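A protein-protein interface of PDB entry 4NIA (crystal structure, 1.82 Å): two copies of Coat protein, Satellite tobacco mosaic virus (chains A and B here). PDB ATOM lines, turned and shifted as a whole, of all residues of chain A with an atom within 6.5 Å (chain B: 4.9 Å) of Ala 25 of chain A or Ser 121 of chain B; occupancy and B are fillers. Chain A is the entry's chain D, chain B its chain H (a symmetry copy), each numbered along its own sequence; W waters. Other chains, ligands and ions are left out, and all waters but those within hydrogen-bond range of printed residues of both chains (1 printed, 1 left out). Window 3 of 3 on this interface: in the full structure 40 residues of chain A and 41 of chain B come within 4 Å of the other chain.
Water W1 bridges OG of Ser 121 of chain B (2.8 Å) and O of Gly 26 of chain A (3.4 Å).
No position is printed for both chains.
Of the 6 pairs that touch across the chains among the printed residues, none has its exchanged pair printed and touching as well.
Ser 27 of chain A touches Trp 81 of chain B.
Printed residues of chain B that touch a printed residue of chain A: Trp 81, Ser 121 and Gly 123.
Hydrophobic or aromatic side chains of chain A within 4 Å of the printed part of chain B: Ile 23, Ala 25 and Tyr 28.
Of the printed residues of chain B, Ile 23 of chain A touches Gly 123.
Ala 25 of chain A touches one residue of chain B.
Of the printed residues of chain B, Gly 26 of chain A touches Trp 81 and Ser 121.
Ser 121 of chain B touches two residues of chain A.
The nearest residue of chain B that does not touch Ala 25 of chain A is Val 122 of chain B (4.05 Å).
The nearest printed residue of chain A that does not touch Ser 121 of chain B is Ser 27 of chain A (5.2 Å).
The nearest printed residue of chain B that does not touch Ser 27 of chain A is Ser 121 of chain B (5.2 Å).
N of Ile 23 of chain A is in hydrogen-bond range of O of Gly 123 of chain B.
The backbone carbonyl oxygen of Ala 25 of chain A lies within hydrogen-bond range of the side-chain hydroxyl of Ser 121 of chain B (3.0 Å).
O of Gly 26 of chain A is in hydrogen-bond range of NE1 of Trp 81 of chain B, 2.8 Å away.
The backbone carbonyl oxygen (O) of Gly 26 of chain A lies within hydrogen-bond range of the side-chain hydroxyl (OG) of Ser 121 of chain B (3.0 Å).
The backbone NH (N) of Tyr 28 of chain A lies close to the indole nitrogen (NE1) of Trp 81 of chain B, 3.3 Å away.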
ATOM      1  N   ILE A  23       7.972  10.102  33.854  1.00  0.00           N
ATOM      2  CA  ILE A  23       7.300  11.303  33.319  1.00  0.00           C
ATOM      3  C   ILE A  23       6.532  10.881  32.073  1.00  0.00           C
ATOM      4  O   ILE A  23       7.083  10.211  31.181  1.00  0.00           O
ATOM      5  CB  ILE A  23       8.328  12.327  32.797  1.00  0.00           C
ATOM      6  CG1 ILE A  23       9.080  12.970  33.952  1.00  0.00           C
ATOM      7  CG2 ILE A  23       7.642  13.411  31.986  1.00  0.00           C
ATOM      8  CD1 ILE A  23      10.206  13.852  33.490  1.00  0.00           C
ATOM      9  N   ARG A  24       5.266  11.268  31.995  1.00  0.00           N
ATOM     10  CA  ARG A  24       4.411  10.858  30.876  1.00  0.00           C
ATOM     11  C   ARG A  24       4.476  11.917  29.783  1.00  0.00           C
ATOM     12  O   ARG A  24       3.518  12.645  29.542  1.00  0.00           O
ATOM     13  CB  ARG A  24       2.968  10.604  31.340  1.00  0.00           C
ATOM     14  CG  ARG A  24       2.885   9.381  32.239  1.00  0.00           C
ATOM     15  CD  ARG A  24       1.480   9.052  32.714  1.00  0.00           C
ATOM     16  NE  ARG A  24       1.439   7.708  33.293  1.00  0.00           N
ATOM     17  CZ  ARG A  24       2.035   7.362  34.432  1.00  0.00           C
ATOM     18  NH1 ARG A  24       2.717   8.258  35.137  1.00  0.00           N
ATOM     19  NH2 ARG A  24       1.949   6.114  34.876  1.00  0.00           N
ATOM     20  N   ALA A  25       5.633  11.965  29.134  1.00  0.00           N
ATOM     21  CA  ALA A  25       5.955  12.920  28.076  1.00  0.00           C
ATOM     22  C   ALA A  25       4.946  12.835  26.938  1.00  0.00           C
ATOM     23  O   ALA A  25       4.405  11.769  26.646  1.00  0.00           O
ATOM     24  CB  ALA A  25       7.368  12.632  27.536  1.00  0.00           C
ATOM     25  N   GLY A  26       4.725  13.971  26.301  1.00  0.00           N
ATOM     26  CA  GLY A  26       3.792  14.078  25.176  1.00  0.00           C
ATOM     27  C   GLY A  26       4.537  14.278  23.871  1.00  0.00           C
ATOM     28  O   GLY A  26       5.507  13.552  23.551  1.00  0.00           O
ATOM     29  N   SER A  27       4.088  15.265  23.111  1.00  0.00           N
ATOM     30  CA  SER A  27       4.678  15.598  21.817  1.00  0.00           C
ATOM     31  C   SER A  27       6.026  16.286  21.965  1.00  0.00           C
ATOM     32  O   SER A  27       6.331  16.846  23.021  1.00  0.00           O
ATOM     33  CB  SER A  27       3.732  16.519  21.046  1.00  0.00           C
ATOM     34  OG  SER A  27       2.501  15.868  20.799  1.00  0.00           O
ATOM     35  N   TYR A  28       6.823  16.286  20.896  1.00  0.00           N
ATOM     36  CA  TYR A  28       8.123  16.933  20.942  1.00  0.00           C
ATOM     37  C   TYR A  28       7.916  18.445  21.110  1.00  0.00           C
ATOM     38  O   TYR A  28       7.171  19.050  20.377  1.00  0.00           O
ATOM     39  CB  TYR A  28       8.923  16.632  19.670  1.00  0.00           C
ATOM     40  CG  TYR A  28      10.358  17.068  19.782  1.00  0.00           C
ATOM     41  CD1 TYR A  28      11.319  16.248  20.362  1.00  0.00           C
ATOM     42  CD2 TYR A  28      10.725  18.356  19.438  1.00  0.00           C
ATOM     43  CE1 TYR A  28      12.628  16.687  20.542  1.00  0.00           C
ATOM     44  CE2 TYR A  28      12.013  18.801  19.636  1.00  0.00           C
ATOM     45  CZ  TYR A  28      12.961  17.977  20.185  1.00  0.00           C
ATOM     46  OH  TYR A  28      14.234  18.431  20.345  1.00  0.00           O
ATOM     47  N   ARG B  79      13.910  13.383  29.029  1.00  0.00           N
ATOM     48  CA  ARG B  79      12.802  12.998  28.163  1.00  0.00           C
ATOM     49  C   ARG B  79      13.375  12.585  26.817  1.00  0.00           C
ATOM     50  O   ARG B  79      14.353  13.163  26.363  1.00  0.00           O
ATOM     51  CB  ARG B  79      11.782  14.136  28.012  1.00  0.00           C
ATOM     52  CG  ARG B  79      11.016  14.477  29.276  1.00  0.00           C
ATOM     53  CD  ARG B  79      10.056  15.658  29.086  1.00  0.00           C
ATOM     54  NE  ARG B  79      10.778  16.914  28.899  1.00  0.00           N
ATOM     55  CZ  ARG B  79      10.253  18.000  28.343  1.00  0.00           C
ATOM     56  NH1 ARG B  79       8.996  17.999  27.921  1.00  0.00           N
ATOM     57  NH2 ARG B  79      10.990  19.087  28.202  1.00  0.00           N
ATOM     58  N   ALA B  80      12.759  11.577  26.195  1.00  0.00           N
ATOM     59  CA  ALA B  80      13.223  11.042  24.934  1.00  0.00           C
ATOM     60  C   ALA B  80      12.054  10.802  23.971  1.00  0.00           C
ATOM     61  O   ALA B  80      10.971  10.386  24.380  1.00  0.00           O
ATOM     62  CB  ALA B  80      13.963   9.749  25.151  1.00  0.00           C
ATOM     63  N   TRP B  81      12.312  11.112  22.717  1.00  0.00           N
ATOM     64  CA  TRP B  81      11.382  10.865  21.579  1.00  0.00           C
ATOM     65  C   TRP B  81      12.086  10.097  20.484  1.00  0.00           C
ATOM     66  O   TRP B  81      13.234  10.339  20.226  1.00  0.00           O
ATOM     67  CB  TRP B  81      10.891  12.186  20.984  1.00  0.00           C
ATOM     68  CG  TRP B  81       9.996  12.975  21.841  1.00  0.00           C
ATOM     69  CD1 TRP B  81       8.644  13.027  21.767  1.00  0.00           C
ATOM     70  CD2 TRP B  81      10.374  13.823  22.938  1.00  0.00           C
ATOM     71  NE1 TRP B  81       8.145  13.845  22.749  1.00  0.00           N
ATOM     72  CE2 TRP B  81       9.183  14.355  23.479  1.00  0.00           C
ATOM     73  CE3 TRP B  81      11.602  14.218  23.482  1.00  0.00           C
ATOM     74  CZ2 TRP B  81       9.175  15.242  24.548  1.00  0.00           C
ATOM     75  CZ3 TRP B  81      11.597  15.106  24.561  1.00  0.00           C
ATOM     76  CH2 TRP B  81      10.375  15.599  25.084  1.00  0.00           C
ATOM     77  N   VAL B  94      10.412   3.643  22.588  1.00  0.00           N
ATOM     78  CA  VAL B  94      11.678   4.026  23.215  1.00  0.00           C
ATOM     79  C   VAL B  94      11.661   3.607  24.674  1.00  0.00           C
ATOM     80  O   VAL B  94      10.623   3.675  25.335  1.00  0.00           O
ATOM     81  CB  VAL B  94      11.925   5.555  23.053  1.00  0.00           C
ATOM     82  CG1 VAL B  94      10.802   6.380  23.681  1.00  0.00           C
ATOM     83  CG2 VAL B  94      13.285   5.940  23.600  1.00  0.00           C
ATOM     84  N   GLY B 111       7.861   4.150  26.406  1.00  0.00           N
ATOM     85  CA  GLY B 111       6.706   4.669  25.674  1.00  0.00           C
ATOM     86  C   GLY B 111       6.627   4.056  24.289  1.00  0.00           C
ATOM     87  O   GLY B 111       7.646   3.734  23.671  1.00  0.00           O
ATOM     88  N   ARG B 112       5.397   3.871  23.820  1.00  0.00           N
ATOM     89  CA  ARG B 112       5.141   3.364  22.479  1.00  0.00           C
ATOM     90  C   ARG B 112       4.168   4.305  21.771  1.00  0.00           C
ATOM     91  O   ARG B 112       3.255   4.842  22.396  1.00  0.00           O
ATOM     92  CB  ARG B 112       4.515   1.954  22.482  1.00  0.00           C
ATOM     93  CG  ARG B 112       5.283   0.941  23.305  1.00  0.00           C
ATOM     94  CD  ARG B 112       4.720  -0.438  23.130  1.00  0.00           C
ATOM     95  NE  ARG B 112       5.361  -1.373  24.053  1.00  0.00           N
ATOM     96  CZ  ARG B 112       5.015  -2.642  24.210  1.00  0.00           C
ATOM     97  NH1 ARG B 112       4.021  -3.167  23.501  1.00  0.00           N
ATOM     98  NH2 ARG B 112       5.668  -3.375  25.082  1.00  0.00           N
ATOM     99  N   ARG B 119       5.709   9.892  16.823  1.00  0.00           N
ATOM    100  CA  ARG B 119       6.822   9.608  17.736  1.00  0.00           C
ATOM    101  C   ARG B 119       6.348   8.894  18.982  1.00  0.00           C
ATOM    102  O   ARG B 119       5.269   9.164  19.463  1.00  0.00           O
ATOM    103  CB  ARG B 119       7.489  10.885  18.216  1.00  0.00           C
ATOM    104  CG  ARG B 119       8.130  11.728  17.103  1.00  0.00           C
ATOM    105  CD  ARG B 119       8.667  13.024  17.698  1.00  0.00           C
ATOM    106  NE  ARG B 119       9.157  13.944  16.666  1.00  0.00           N
ATOM    107  CZ  ARG B 119      10.439  14.156  16.383  1.00  0.00           C
ATOM    108  NH1 ARG B 119      11.401  13.521  17.053  1.00  0.00           N
ATOM    109  NH2 ARG B 119      10.767  15.084  15.487  1.00  0.00           N
ATOM    110  N   ALA B 120       7.178   7.985  19.484  1.00  0.00           N
ATOM    111  CA  ALA B 120       7.028   7.429  20.826  1.00  0.00           C
ATOM    112  C   ALA B 120       7.841   8.304  21.766  1.00  0.00           C
ATOM    113  O   ALA B 120       8.862   8.861  21.352  1.00  0.00           O
ATOM    114  CB  ALA B 120       7.545   6.027  20.882  1.00  0.00           C
ATOM    115  N   SER B 121       7.359   8.461  22.987  1.00  0.00           N
ATOM    116  CA  SER B 121       8.069   9.263  23.987  1.00  0.00           C
ATOM    117  C   SER B 121       7.948   8.705  25.387  1.00  0.00           C
ATOM    118  O   SER B 121       6.980   8.023  25.732  1.00  0.00           O
ATOM    119  CB  SER B 121       7.559  10.701  23.949  1.00  0.00           C
ATOM    120  OG  SER B 121       6.222  10.765  24.424  1.00  0.00           O
ATOM    121  N   VAL B 122       8.918   9.041  26.230  1.00  0.00           N
ATOM    122  CA  VAL B 122       8.856   8.701  27.642  1.00  0.00           C
ATOM    123  C   VAL B 122       9.899   9.577  28.337  1.00  0.00           C
ATOM    124  O   VAL B 122      10.774  10.160  27.682  1.00  0.00           O
ATOM    125  CB  VAL B 122       9.131   7.199  27.915  1.00  0.00           C
ATOM    126  CG1 VAL B 122      10.586   6.839  27.733  1.00  0.00           C
ATOM    127  CG2 VAL B 122       8.614   6.773  29.286  1.00  0.00           C
ATOM    128  N   GLY B 123       9.787   9.703  29.650  1.00  0.00           N
ATOM    129  CA  GLY B 123      10.856  10.334  30.398  1.00  0.00           C
ATOM    130  C   GLY B 123      10.924   9.868  31.827  1.00  0.00           C
ATOM    131  O   GLY B 123      10.059   9.109  32.277  1.00  0.00           O
HETATM  132  O   HOH W   1       3.768  10.712  23.129  1.00  0.00           O
